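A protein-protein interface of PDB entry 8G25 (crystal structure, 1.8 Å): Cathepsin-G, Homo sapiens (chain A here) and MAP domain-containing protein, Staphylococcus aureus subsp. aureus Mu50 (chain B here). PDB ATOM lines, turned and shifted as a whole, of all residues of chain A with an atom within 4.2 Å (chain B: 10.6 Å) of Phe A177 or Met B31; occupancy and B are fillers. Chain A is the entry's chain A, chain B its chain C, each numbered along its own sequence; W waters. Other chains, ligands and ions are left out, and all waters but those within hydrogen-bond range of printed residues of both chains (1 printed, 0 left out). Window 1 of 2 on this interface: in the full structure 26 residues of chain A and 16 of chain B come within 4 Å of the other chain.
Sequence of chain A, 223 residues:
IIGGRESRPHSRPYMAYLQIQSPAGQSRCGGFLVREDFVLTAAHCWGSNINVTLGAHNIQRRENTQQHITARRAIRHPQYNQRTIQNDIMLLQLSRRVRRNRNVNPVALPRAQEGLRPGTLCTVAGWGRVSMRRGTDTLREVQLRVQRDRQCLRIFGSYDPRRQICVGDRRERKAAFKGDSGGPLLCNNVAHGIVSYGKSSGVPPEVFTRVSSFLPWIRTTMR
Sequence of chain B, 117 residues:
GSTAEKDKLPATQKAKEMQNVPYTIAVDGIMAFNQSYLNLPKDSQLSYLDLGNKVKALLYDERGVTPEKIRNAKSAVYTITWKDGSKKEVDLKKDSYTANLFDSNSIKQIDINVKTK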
ATOM      1  N   ILE A   2     -20.942 -17.782 -23.210  1.00  0.00           N
ATOM      2  CA  ILE A   2     -20.293 -17.401 -24.461  1.00  0.00           C
ATOM      3  C   ILE A   2     -19.862 -15.948 -24.341  1.00  0.00           C
ATOM      4  O   ILE A   2     -20.663 -15.084 -23.953  1.00  0.00           O
ATOM      5  CB  ILE A   2     -21.235 -17.584 -25.667  1.00  0.00           C
ATOM      6  CG1 ILE A   2     -21.705 -19.033 -25.796  1.00  0.00           C
ATOM      7  CG2 ILE A   2     -20.572 -17.128 -26.948  1.00  0.00           C
ATOM      8  CD1 ILE A   2     -22.812 -19.220 -26.826  1.00  0.00           C
ATOM      9  N   ARG A 129     -20.874 -24.380 -21.361  1.00  0.00           N
ATOM     10  CA  ARG A 129     -19.927 -24.373 -22.469  1.00  0.00           C
ATOM     11  C   ARG A 129     -19.712 -22.959 -22.996  1.00  0.00           C
ATOM     12  O   ARG A 129     -20.603 -22.102 -22.939  1.00  0.00           O
ATOM     13  CB  ARG A 129     -20.429 -25.281 -23.594  1.00  0.00           C
ATOM     14  CG  ARG A 129     -20.665 -26.727 -23.159  1.00  0.00           C
ATOM     15  CD  ARG A 129     -20.740 -27.675 -24.344  1.00  0.00           C
ATOM     16  NE  ARG A 129     -19.428 -27.940 -24.927  1.00  0.00           N
ATOM     17  CZ  ARG A 129     -18.516 -28.748 -24.402  1.00  0.00           C
ATOM     18  NH1 ARG A 129     -18.724 -29.377 -23.256  1.00  0.00           N
ATOM     19  NH2 ARG A 129     -17.363 -28.930 -25.042  1.00  0.00           N
ATOM     20  N   SER A 131     -18.523 -22.474 -26.197  1.00  0.00           N
ATOM     21  CA  SER A 131     -18.645 -22.593 -27.642  1.00  0.00           C
ATOM     22  C   SER A 131     -19.262 -23.956 -27.910  1.00  0.00           C
ATOM     23  O   SER A 131     -19.505 -24.738 -26.984  1.00  0.00           O
ATOM     24  CB  SER A 131     -17.293 -22.445 -28.341  1.00  0.00           C
ATOM     25  OG  SER A 131     -16.416 -23.510 -27.995  1.00  0.00           O
ATOM     26  N   ALA A 175     -23.565 -14.389 -24.267  1.00  0.00           N
ATOM     27  CA  ALA A 175     -24.809 -15.038 -23.876  1.00  0.00           C
ATOM     28  C   ALA A 175     -24.495 -16.150 -22.889  1.00  0.00           C
ATOM     29  O   ALA A 175     -23.347 -16.579 -22.747  1.00  0.00           O
ATOM     30  CB  ALA A 175     -25.557 -15.601 -25.091  1.00  0.00           C
ATOM     31  N   ALA A 176     -25.541 -16.608 -22.213  1.00  0.00           N
ATOM     32  CA  ALA A 176     -25.530 -17.877 -21.513  1.00  0.00           C
ATOM     33  C   ALA A 176     -25.710 -19.007 -22.520  1.00  0.00           C
ATOM     34  O   ALA A 176     -26.207 -18.806 -23.631  1.00  0.00           O
ATOM     35  CB  ALA A 176     -26.631 -17.912 -20.446  1.00  0.00           C
ATOM     36  N   PHE A 177     -25.291 -20.205 -22.135  1.00  0.00           N
ATOM     37  CA  PHE A 177     -25.317 -21.306 -23.094  1.00  0.00           C
ATOM     38  C   PHE A 177     -25.511 -22.610 -22.330  1.00  0.00           C
ATOM     39  O   PHE A 177     -25.880 -22.594 -21.154  1.00  0.00           O
ATOM     40  CB  PHE A 177     -24.045 -21.300 -23.950  1.00  0.00           C
ATOM     41  CG  PHE A 177     -24.201 -22.026 -25.251  1.00  0.00           C
ATOM     42  CD1 PHE A 177     -25.354 -21.867 -26.005  1.00  0.00           C
ATOM     43  CD2 PHE A 177     -23.212 -22.858 -25.719  1.00  0.00           C
ATOM     44  CE1 PHE A 177     -25.499 -22.534 -27.208  1.00  0.00           C
ATOM     45  CE2 PHE A 177     -23.355 -23.516 -26.916  1.00  0.00           C
ATOM     46  CZ  PHE A 177     -24.504 -23.355 -27.654  1.00  0.00           C
ATOM     47  N   LYS A 178     -25.224 -23.738 -22.991  1.00  0.00           N
ATOM     48  CA  LYS A 178     -25.520 -25.063 -22.452  1.00  0.00           C
ATOM     49  C   LYS A 178     -24.780 -25.326 -21.143  1.00  0.00           C
ATOM     50  O   LYS A 178     -23.546 -25.367 -21.119  1.00  0.00           O
ATOM     51  CB  LYS A 178     -25.141 -26.125 -23.485  1.00  0.00           C
ATOM     52  CG  LYS A 178     -26.065 -26.188 -24.683  1.00  0.00           C
ATOM     53  CD  LYS A 178     -25.370 -26.777 -25.899  1.00  0.00           C
ATOM     54  CE  LYS A 178     -24.518 -27.984 -25.542  1.00  0.00           C
ATOM     55  NZ  LYS A 178     -23.876 -28.602 -26.736  1.00  0.00           N
ATOM     56  N   GLY A 179     -25.537 -25.583 -20.074  1.00  0.00           N
ATOM     57  CA  GLY A 179     -24.989 -25.821 -18.749  1.00  0.00           C
ATOM     58  C   GLY A 179     -25.128 -24.646 -17.803  1.00  0.00           C
ATOM     59  O   GLY A 179     -24.915 -24.811 -16.594  1.00  0.00           O
ATOM     60  N   ASP A 180     -25.478 -23.472 -18.321  1.00  0.00           N
ATOM     61  CA  ASP A 180     -25.740 -22.277 -17.527  1.00  0.00           C
ATOM     62  C   ASP A 180     -27.175 -22.163 -17.044  1.00  0.00           C
ATOM     63  O   ASP A 180     -27.452 -21.292 -16.216  1.00  0.00           O
ATOM     64  CB  ASP A 180     -25.422 -21.020 -18.334  1.00  0.00           C
ATOM     65  CG  ASP A 180     -23.972 -20.909 -18.673  1.00  0.00           C
ATOM     66  OD1 ASP A 180     -23.144 -21.235 -17.798  1.00  0.00           O
ATOM     67  OD2 ASP A 180     -23.666 -20.512 -19.818  1.00  0.00           O
ATOM     68  N   TYR A 197     -33.647 -20.381 -21.489  1.00  0.00           N
ATOM     69  CA  TYR A 197     -33.557 -20.977 -22.820  1.00  0.00           C
ATOM     70  C   TYR A 197     -33.188 -19.917 -23.843  1.00  0.00           C
ATOM     71  O   TYR A 197     -33.091 -18.733 -23.531  1.00  0.00           O
ATOM     72  CB  TYR A 197     -34.856 -21.708 -23.196  1.00  0.00           C
ATOM     73  CG  TYR A 197     -36.101 -20.866 -23.459  1.00  0.00           C
ATOM     74  CD1 TYR A 197     -36.278 -20.210 -24.680  1.00  0.00           C
ATOM     75  CD2 TYR A 197     -37.133 -20.797 -22.523  1.00  0.00           C
ATOM     76  CE1 TYR A 197     -37.412 -19.476 -24.948  1.00  0.00           C
ATOM     77  CE2 TYR A 197     -38.289 -20.053 -22.783  1.00  0.00           C
ATOM     78  CZ  TYR A 197     -38.415 -19.399 -24.005  1.00  0.00           C
ATOM     79  OH  TYR A 197     -39.551 -18.659 -24.287  1.00  0.00           O
ATOM     80  N   GLY A 198     -32.920 -20.372 -25.062  1.00  0.00           N
ATOM     81  CA  GLY A 198     -32.625 -19.462 -26.138  1.00  0.00           C
ATOM     82  C   GLY A 198     -32.495 -20.246 -27.425  1.00  0.00           C
ATOM     83  O   GLY A 198     -33.001 -21.364 -27.540  1.00  0.00           O
ATOM     84  N   SER A 200     -30.540 -22.409 -30.300  1.00  0.00           N
ATOM     85  CA  SER A 200     -29.536 -23.460 -30.198  1.00  0.00           C
ATOM     86  C   SER A 200     -28.157 -22.988 -30.638  1.00  0.00           C
ATOM     87  O   SER A 200     -27.160 -23.637 -30.310  1.00  0.00           O
ATOM     88  CB  SER A 200     -29.943 -24.690 -31.014  1.00  0.00           C
ATOM     89  OG  SER A 200     -29.900 -24.407 -32.399  1.00  0.00           O
ATOM     90  N   SER A 201     -28.075 -21.879 -31.371  1.00  0.00           N
ATOM     91  CA  SER A 201     -26.794 -21.324 -31.784  1.00  0.00           C
ATOM     92  C   SER A 201     -26.095 -20.540 -30.681  1.00  0.00           C
ATOM     93  O   SER A 201     -24.905 -20.230 -30.821  1.00  0.00           O
ATOM     94  CB  SER A 201     -27.001 -20.401 -32.985  1.00  0.00           C
ATOM     95  OG  SER A 201     -27.917 -19.372 -32.637  1.00  0.00           O
ATOM     96  N   GLY A 202     -26.805 -20.185 -29.620  1.00  0.00           N
ATOM     97  CA  GLY A 202     -26.288 -19.303 -28.598  1.00  0.00           C
ATOM     98  C   GLY A 202     -26.354 -17.830 -28.933  1.00  0.00           C
ATOM     99  O   GLY A 202     -26.023 -17.004 -28.073  1.00  0.00           O
ATOM    100  N   PRO B  22     -23.250 -36.727 -24.961  1.00  0.00           N
ATOM    101  CA  PRO B  22     -23.991 -35.462 -24.920  1.00  0.00           C
ATOM    102  C   PRO B  22     -25.061 -35.399 -26.004  1.00  0.00           C
ATOM    103  O   PRO B  22     -24.898 -35.917 -27.119  1.00  0.00           O
ATOM    104  CB  PRO B  22     -22.901 -34.398 -25.125  1.00  0.00           C
ATOM    105  CG  PRO B  22     -21.741 -35.130 -25.725  1.00  0.00           C
ATOM    106  CD  PRO B  22     -21.812 -36.538 -25.231  1.00  0.00           C
ATOM    107  N   TYR B  23     -26.176 -34.755 -25.661  1.00  0.00           N
ATOM    108  CA  TYR B  23     -27.225 -34.536 -26.641  1.00  0.00           C
ATOM    109  C   TYR B  23     -27.867 -33.178 -26.385  1.00  0.00           C
ATOM    110  O   TYR B  23     -27.824 -32.637 -25.275  1.00  0.00           O
ATOM    111  CB  TYR B  23     -28.302 -35.650 -26.612  1.00  0.00           C
ATOM    112  CG  TYR B  23     -29.127 -35.664 -25.350  1.00  0.00           C
ATOM    113  CD1 TYR B  23     -30.275 -34.878 -25.233  1.00  0.00           C
ATOM    114  CD2 TYR B  23     -28.758 -36.443 -24.258  1.00  0.00           C
ATOM    115  CE1 TYR B  23     -31.021 -34.878 -24.076  1.00  0.00           C
ATOM    116  CE2 TYR B  23     -29.501 -36.439 -23.094  1.00  0.00           C
ATOM    117  CZ  TYR B  23     -30.635 -35.655 -23.010  1.00  0.00           C
ATOM    118  OH  TYR B  23     -31.379 -35.648 -21.854  1.00  0.00           O
ATOM    119  N   THR B  24     -28.450 -32.624 -27.435  1.00  0.00           N
ATOM    120  CA  THR B  24     -29.226 -31.399 -27.301  1.00  0.00           C
ATOM    121  C   THR B  24     -30.588 -31.611 -27.931  1.00  0.00           C
ATOM    122  O   THR B  24     -30.737 -32.429 -28.836  1.00  0.00           O
ATOM    123  CB  THR B  24     -28.564 -30.206 -27.967  1.00  0.00           C
ATOM    124  OG1 THR B  24     -28.500 -30.446 -29.377  1.00  0.00           O
ATOM    125  CG2 THR B  24     -27.166 -29.988 -27.417  1.00  0.00           C
ATOM    126  N   ILE B  25     -31.578 -30.864 -27.448  1.00  0.00           N
ATOM    127  CA  ILE B  25     -32.923 -30.892 -28.009  1.00  0.00           C
ATOM    128  C   ILE B  25     -33.318 -29.463 -28.336  1.00  0.00           C
ATOM    129  O   ILE B  25     -33.280 -28.594 -27.460  1.00  0.00           O
ATOM    130  CB  ILE B  25     -33.947 -31.518 -27.047  1.00  0.00           C
ATOM    131  CG1 ILE B  25     -33.489 -32.908 -26.597  1.00  0.00           C
ATOM    132  CG2 ILE B  25     -35.311 -31.602 -27.718  1.00  0.00           C
ATOM    133  CD1 ILE B  25     -34.363 -33.504 -25.514  1.00  0.00           C
ATOM    134  N   ALA B  26     -33.690 -29.219 -29.590  1.00  0.00           N
ATOM    135  CA  ALA B  26     -34.320 -27.973 -30.002  1.00  0.00           C
ATOM    136  C   ALA B  26     -35.697 -28.297 -30.560  1.00  0.00           C
ATOM    137  O   ALA B  26     -35.835 -29.177 -31.418  1.00  0.00           O
ATOM    138  CB  ALA B  26     -33.471 -27.233 -31.034  1.00  0.00           C
ATOM    139  N   VAL B  27     -36.718 -27.619 -30.051  1.00  0.00           N
ATOM    140  CA  VAL B  27     -38.072 -27.749 -30.568  1.00  0.00           C
ATOM    141  C   VAL B  27     -38.571 -26.352 -30.901  1.00  0.00           C
ATOM    142  O   VAL B  27     -38.626 -25.483 -30.021  1.00  0.00           O
ATOM    143  CB  VAL B  27     -39.009 -28.444 -29.570  1.00  0.00           C
ATOM    144  CG1 VAL B  27     -40.405 -28.625 -30.175  1.00  0.00           C
ATOM    145  CG2 VAL B  27     -38.415 -29.780 -29.121  1.00  0.00           C
ATOM    146  N   ASP B  28     -38.928 -26.138 -32.169  1.00  0.00           N
ATOM    147  CA  ASP B  28     -39.417 -24.844 -32.646  1.00  0.00           C
ATOM    148  C   ASP B  28     -38.399 -23.734 -32.390  1.00  0.00           C
ATOM    149  O   ASP B  28     -38.754 -22.622 -31.999  1.00  0.00           O
ATOM    150  CB  ASP B  28     -40.767 -24.505 -32.014  1.00  0.00           C
ATOM    151  CG  ASP B  28     -41.842 -25.509 -32.376  1.00  0.00           C
ATOM    152  OD1 ASP B  28     -41.951 -25.854 -33.572  1.00  0.00           O
ATOM    153  OD2 ASP B  28     -42.572 -25.959 -31.465  1.00  0.00           O
ATOM    154  N   GLY B  29     -37.119 -24.045 -32.592  1.00  0.00           N
ATOM    155  CA  GLY B  29     -36.062 -23.063 -32.465  1.00  0.00           C
ATOM    156  C   GLY B  29     -35.655 -22.710 -31.049  1.00  0.00           C
ATOM    157  O   GLY B  29     -34.807 -21.824 -30.872  1.00  0.00           O
ATOM    158  N   ILE B  30     -36.219 -23.368 -30.037  1.00  0.00           N
ATOM    159  CA  ILE B  30     -35.947 -23.057 -28.638  1.00  0.00           C
ATOM    160  C   ILE B  30     -35.202 -24.230 -28.017  1.00  0.00           C
ATOM    161  O   ILE B  30     -35.634 -25.380 -28.138  1.00  0.00           O
ATOM    162  CB  ILE B  30     -37.244 -22.755 -27.860  1.00  0.00           C
ATOM    163  CG1 ILE B  30     -37.691 -21.305 -28.066  1.00  0.00           C
ATOM    164  CG2 ILE B  30     -37.066 -23.026 -26.397  1.00  0.00           C
ATOM    165  CD1 ILE B  30     -38.468 -21.057 -29.332  1.00  0.00           C
ATOM    166  N   MET B  31     -34.085 -23.936 -27.351  1.00  0.00           N
ATOM    167  CA  MET B  31     -33.285 -24.943 -26.662  1.00  0.00           C
ATOM    168  C   MET B  31     -33.078 -24.539 -25.209  1.00  0.00           C
ATOM    169  O   MET B  31     -32.559 -23.456 -24.935  1.00  0.00           O
ATOM    170  CB  MET B  31     -31.932 -25.125 -27.356  1.00  0.00           C
ATOM    171  CG  MET B  31     -31.015 -26.107 -26.673  1.00  0.00           C
ATOM    172  SD  MET B  31     -29.535 -26.374 -27.682  1.00  0.00           S
ATOM    173  CE  MET B  31     -28.508 -24.988 -27.184  1.00  0.00           C
ATOM    174  N   ALA B  32     -33.463 -25.418 -24.286  1.00  0.00           N
ATOM    175  CA  ALA B  32     -33.154 -25.204 -22.882  1.00  0.00           C
ATOM    176  C   ALA B  32     -31.643 -25.266 -22.680  1.00  0.00           C
ATOM    177  O   ALA B  32     -30.933 -25.985 -23.379  1.00  0.00           O
ATOM    178  CB  ALA B  32     -33.852 -26.252 -22.012  1.00  0.00           C
ATOM    179  N   PHE B  33     -31.141 -24.476 -21.735  1.00  0.00           N
ATOM    180  CA  PHE B  33     -29.700 -24.309 -21.616  1.00  0.00           C
ATOM    181  C   PHE B  33     -29.086 -25.207 -20.536  1.00  0.00           C
ATOM    182  O   PHE B  33     -28.106 -24.825 -19.889  1.00  0.00           O
ATOM    183  CB  PHE B  33     -29.368 -22.842 -21.372  1.00  0.00           C
ATOM    184  CG  PHE B  33     -29.351 -22.004 -22.629  1.00  0.00           C
ATOM    185  CD1 PHE B  33     -29.284 -22.603 -23.890  1.00  0.00           C
ATOM    186  CD2 PHE B  33     -29.393 -20.624 -22.553  1.00  0.00           C
ATOM    187  CE1 PHE B  33     -29.255 -21.837 -25.049  1.00  0.00           C
ATOM    188  CE2 PHE B  33     -29.369 -19.847 -23.707  1.00  0.00           C
ATOM    189  CZ  PHE B  33     -29.299 -20.457 -24.965  1.00  0.00           C
ATOM    190  N   ASN B  34     -29.663 -26.385 -20.291  1.00  0.00           N
ATOM    191  CA  ASN B  34     -28.933 -27.356 -19.489  1.00  0.00           C
ATOM    192  C   ASN B  34     -27.923 -28.089 -20.376  1.00  0.00           C
ATOM    193  O   ASN B  34     -27.902 -27.927 -21.593  1.00  0.00           O
ATOM    194  CB  ASN B  34     -29.889 -28.336 -18.811  1.00  0.00           C
ATOM    195  CG  ASN B  34     -30.785 -29.059 -19.794  1.00  0.00           C
ATOM    196  OD1 ASN B  34     -30.907 -28.663 -20.951  1.00  0.00           O
ATOM    197  ND2 ASN B  34     -31.433 -30.114 -19.328  1.00  0.00           N
ATOM    198  N   GLN B  35     -27.070 -28.904 -19.758  1.00  0.00           N
ATOM    199  CA  GLN B  35     -26.080 -29.695 -20.487  1.00  0.00           C
ATOM    200  C   GLN B  35     -26.305 -31.162 -20.136  1.00  0.00           C
ATOM    201  O   GLN B  35     -25.998 -31.590 -19.019  1.00  0.00           O
ATOM    202  CB  GLN B  35     -24.665 -29.238 -20.139  1.00  0.00           C
ATOM    203  CG  GLN B  35     -23.549 -29.961 -20.868  1.00  0.00           C
ATOM    204  CD  GLN B  35     -22.206 -29.276 -20.658  1.00  0.00           C
ATOM    205  OE1 GLN B  35     -22.065 -28.424 -19.775  1.00  0.00           O
ATOM    206  NE2 GLN B  35     -21.219 -29.637 -21.471  1.00  0.00           N
ATOM    207  N   SER B  36     -26.851 -31.933 -21.072  1.00  0.00           N
ATOM    208  CA  SER B  36     -27.363 -33.256 -20.739  1.00  0.00           C
ATOM    209  C   SER B  36     -26.687 -34.353 -21.556  1.00  0.00           C
ATOM    210  O   SER B  36     -26.217 -34.136 -22.681  1.00  0.00           O
ATOM    211  CB  SER B  36     -28.884 -33.329 -20.933  1.00  0.00           C
ATOM    212  OG  SER B  36     -29.561 -32.556 -19.947  1.00  0.00           O
ATOM    213  N   LEU B  59     -37.352 -36.922 -26.126  1.00  0.00           N
ATOM    214  CA  LEU B  59     -38.193 -35.847 -26.634  1.00  0.00           C
ATOM    215  C   LEU B  59     -39.465 -35.717 -25.819  1.00  0.00           C
ATOM    216  O   LEU B  59     -39.873 -34.597 -25.462  1.00  0.00           O
ATOM    217  CB  LEU B  59     -38.514 -36.103 -28.108  1.00  0.00           C
ATOM    218  CG  LEU B  59     -37.539 -35.532 -29.124  1.00  0.00           C
ATOM    219  CD1 LEU B  59     -37.841 -36.157 -30.487  1.00  0.00           C
ATOM    220  CD2 LEU B  59     -37.734 -34.033 -29.152  1.00  0.00           C
ATOM    221  N   GLU B  62     -38.483 -34.723 -21.862  1.00  0.00           N
ATOM    222  CA  GLU B  62     -37.876 -33.425 -21.619  1.00  0.00           C
ATOM    223  C   GLU B  62     -38.649 -32.267 -22.242  1.00  0.00           C
ATOM    224  O   GLU B  62     -38.663 -31.168 -21.669  1.00  0.00           O
ATOM    225  CB  GLU B  62     -36.429 -33.434 -22.112  1.00  0.00           C
ATOM    226  CG  GLU B  62     -35.656 -34.613 -21.522  1.00  0.00           C
ATOM    227  CD  GLU B  62     -34.148 -34.414 -21.486  1.00  0.00           C
ATOM    228  OE1 GLU B  62     -33.649 -33.419 -22.052  1.00  0.00           O
ATOM    229  OE2 GLU B  62     -33.458 -35.260 -20.877  1.00  0.00           O
ATOM    230  N   ARG B  63     -39.302 -32.472 -23.386  1.00  0.00           N
ATOM    231  CA  ARG B  63     -39.987 -31.364 -24.033  1.00  0.00           C
ATOM    232  C   ARG B  63     -41.429 -31.701 -24.375  1.00  0.00           C
ATOM    233  O   ARG B  63     -42.066 -30.946 -25.116  1.00  0.00           O
ATOM    234  CB  ARG B  63     -39.241 -30.914 -25.283  1.00  0.00           C
ATOM    235  CG  ARG B  63     -37.939 -30.174 -25.002  1.00  0.00           C
ATOM    236  CD  ARG B  63     -38.128 -28.881 -24.182  1.00  0.00           C
ATOM    237  NE  ARG B  63     -38.973 -27.903 -24.876  1.00  0.00           N
ATOM    238  CZ  ARG B  63     -38.542 -27.057 -25.803  1.00  0.00           C
ATOM    239  NH1 ARG B  63     -37.271 -27.016 -26.161  1.00  0.00           N
ATOM    240  NH2 ARG B  63     -39.415 -26.238 -26.393  1.00  0.00           N
ATOM    241  N   GLN B 109     -21.946 -37.408 -30.217  1.00  0.00           N
ATOM    242  CA  GLN B 109     -22.930 -36.370 -29.919  1.00  0.00           C
ATOM    243  C   GLN B 109     -24.238 -36.715 -30.617  1.00  0.00           C
ATOM    244  O   GLN B 109     -24.239 -37.370 -31.660  1.00  0.00           O
ATOM    245  CB  GLN B 109     -22.418 -34.995 -30.372  1.00  0.00           C
ATOM    246  CG  GLN B 109     -23.457 -33.879 -30.397  1.00  0.00           C
ATOM    247  CD  GLN B 109     -23.526 -33.101 -29.100  1.00  0.00           C
ATOM    248  OE1 GLN B 109     -22.516 -32.914 -28.421  1.00  0.00           O
ATOM    249  NE2 GLN B 109     -24.723 -32.635 -28.750  1.00  0.00           N
ATOM    250  N   ILE B 110     -25.356 -36.278 -30.034  1.00  0.00           N
ATOM    251  CA  ILE B 110     -26.660 -36.410 -30.673  1.00  0.00           C
ATOM    252  C   ILE B 110     -27.382 -35.071 -30.608  1.00  0.00           C
ATOM    253  O   ILE B 110     -27.495 -34.470 -29.536  1.00  0.00           O
ATOM    254  CB  ILE B 110     -27.514 -37.515 -30.025  1.00  0.00           C
ATOM    255  CG1 ILE B 110     -26.782 -38.861 -30.103  1.00  0.00           C
ATOM    256  CG2 ILE B 110     -28.848 -37.625 -30.743  1.00  0.00           C
ATOM    257  CD1 ILE B 110     -27.416 -39.940 -29.266  1.00  0.00           C
ATOM    258  N   ASP B 111     -27.870 -34.598 -31.750  1.00  0.00           N
ATOM    259  CA  ASP B 111     -28.547 -33.306 -31.807  1.00  0.00           C
ATOM    260  C   ASP B 111     -29.938 -33.509 -32.388  1.00  0.00           C
ATOM    261  O   ASP B 111     -30.077 -33.863 -33.567  1.00  0.00           O
ATOM    262  CB  ASP B 111     -27.721 -32.322 -32.623  1.00  0.00           C
ATOM    263  CG  ASP B 111     -26.408 -31.989 -31.945  1.00  0.00           C
ATOM    264  OD1 ASP B 111     -26.442 -31.455 -30.815  1.00  0.00           O
ATOM    265  OD2 ASP B 111     -25.344 -32.294 -32.517  1.00  0.00           O
ATOM    266  N   ILE B 112     -30.960 -33.266 -31.565  1.00  0.00           N
ATOM    267  CA  ILE B 112     -32.353 -33.531 -31.898  1.00  0.00           C
ATOM    268  C   ILE B 112     -33.018 -32.207 -32.232  1.00  0.00           C
ATOM    269  O   ILE B 112     -32.893 -31.231 -31.482  1.00  0.00           O
ATOM    270  CB  ILE B 112     -33.079 -34.231 -30.738  1.00  0.00           C
ATOM    271  CG1 ILE B 112     -32.313 -35.490 -30.298  1.00  0.00           C
ATOM    272  CG2 ILE B 112     -34.535 -34.544 -31.120  1.00  0.00           C
ATOM    273  CD1 ILE B 112     -32.539 -35.880 -28.831  1.00  0.00           C
ATOM    274  N   ASN B 113     -33.718 -32.161 -33.359  1.00  0.00           N
ATOM    275  CA  ASN B 113     -34.331 -30.921 -33.811  1.00  0.00           C
ATOM    276  C   ASN B 113     -35.713 -31.226 -34.360  1.00  0.00           C
ATOM    277  O   ASN B 113     -35.841 -31.935 -35.362  1.00  0.00           O
ATOM    278  CB  ASN B 113     -33.466 -30.234 -34.870  1.00  0.00           C
ATOM    279  CG  ASN B 113     -33.886 -28.798 -35.120  1.00  0.00           C
ATOM    280  OD1 ASN B 113     -35.005 -28.401 -34.797  1.00  0.00           O
ATOM    281  ND2 ASN B 113     -32.987 -28.010 -35.700  1.00  0.00           N
ATOM    282  N   VAL B 114     -36.738 -30.671 -33.718  1.00  0.00           N
ATOM    283  CA  VAL B 114     -38.122 -30.834 -34.145  1.00  0.00           C
ATOM    284  C   VAL B 114     -38.678 -29.473 -34.514  1.00  0.00           C
ATOM    285  O   VAL B 114     -38.548 -28.513 -33.743  1.00  0.00           O
ATOM    286  CB  VAL B 114     -38.986 -31.492 -33.058  1.00  0.00           C
ATOM    287  CG1 VAL B 114     -40.434 -31.543 -33.513  1.00  0.00           C
ATOM    288  CG2 VAL B 114     -38.472 -32.885 -32.752  1.00  0.00           C
HETATM  289  O   HOH W   1     -26.454 -26.286 -29.400  1.00  0.00           O
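N of Gly A179 lies within hydrogen-bond range of O of Phe B33 (2.7 Å). The guanidinium group (NH1) of Arg A129 sits close to the side-chain amide nitrogen (NE2) of Gln B35. N of Asp A180 lies within hydrogen-bond range of O of Phe B33 (3.3 Å). The backbone carbonyl oxygen (O) of Phe A177 lies close to the backbone carbonyl oxygen (O) of Phe B33 (3.4 Å). N of Met B31 sits at hydrogen-bond distance from O of Gly A198 (2.8 Å).
ND2 of Asn B34 sits at hydrogen-bond distance from OG of Ser B36 (3.1 Å). The backbone carbonyl oxygen of Thr B24 lies within hydrogen-bond range of the backbone NH of Ile B112 (2.9 Å). The backbone carbonyl oxygen of Lys A178 sits at hydrogen-bond distance from the backbone NH of Arg A129 (2.9 Å). The backbone carbonyl oxygen of Ile B110 lies within hydrogen-bond range of the backbone NH of Thr B24, 3.0 Å away. The side-chain hydroxyl of Thr B24 sits at hydrogen-bond distance from the side-chain carboxylate of Asp B111, at 2.7 Å. The backbone carbonyl oxygen (O) of Ile B30 is in hydrogen-bond range of the guanidinium group (NH1) of Arg B63 (3.0 Å).
Lys A178 touches Phe B33. Lys A178 touches Asn B34 (CB to O, 3.8 Å). Gln B35 touches Lys A178. Gly A179 touches Asn B34 (N to C, 3.5 Å). Gly A179 touches Gln B35 (N to N, 3.7 Å). Ile B30 touches Tyr A197 (CG2 to CD1, 3.4 Å). Tyr A197 touches Ala B32 (CB to CA, 3.9 Å). Ile B30 touches Gly A198. N of Gly A198 touches CZ of Phe B33, at 3.6 Å. Ser A200 touches Met B31.
Printed residues of chain B within 4 Å of Arg A129: Gln B35 (3.1 Å). No residue of chain B comes within 4 Å of Ala A175. Of chain B, only Phe B33 comes within 4 Å of Ala A176. Phe A177 touches just these residues of chain B: Met B31 and Phe B33. Lys A178 touches just these residues of chain B: Thr B24 (3.6 Å), Met B31 (3.7 Å), Phe B33 (3.6 Å), Asn B34 (3.8 Å) and Gln B35 (3.7 Å). Printed residues of chain B within 4 Å of Tyr A197: Ile B30 (3.4 Å), Met B31 (3.4 Å), Ala B32 (3.9 Å) and Phe B33 (3.8 Å). Gly A198 touches four residues of chain B. Ser A200 touches one residue of chain B. Ser A201 touches none of the printed residues of chain B. No residue of chain B comes within 4 Å of Gly A202. Printed residues of chain A within 4 Å of Gly B29: Gly A198. Of the printed residues of chain A, Met B31 touches Phe A177, Lys A178, Tyr A197, Gly A198 and Ser A200. Asp B111 touches none of the printed residues of chain A. The nearest residue of chain B that does not touch Phe A177 is Asn B34 (5.4 Å). The nearest printed residue of chain A that does not touch Gln B35 is Asp A180 (5.8 Å).
Of the 24 printed residues of chain B, 8 touch a printed residue of chain A. Hydrophobic or aromatic side chains of chain B that line the printed part of chain A: Ile B30, Met B31 and Phe B33. Of the 14 printed residues of chain A, 9 touch a printed residue of chain B. Printed residues of chain A that touch a printed residue of chain B: Arg A129, Ala A176, Phe A177, Lys A178, Gly A179, Asp A180, Tyr A197, Gly A198 and Ser A200. Hydrophobic or aromatic side chains of chain A that line the printed part of chain B: Phe A177 and Tyr A197. Among the printed residues, 22 pairs touch across the chains. Among the printed residues, no Asp or Glu carboxylate lies within 4 Å of a Lys or Arg side-chain nitrogen of the other chain.
Water W1 lies within hydrogen-bond range of the backbone carbonyl oxygen of Ser A200 (2.9 Å) and the side-chain sulfur of Met B31 (3.5 Å).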
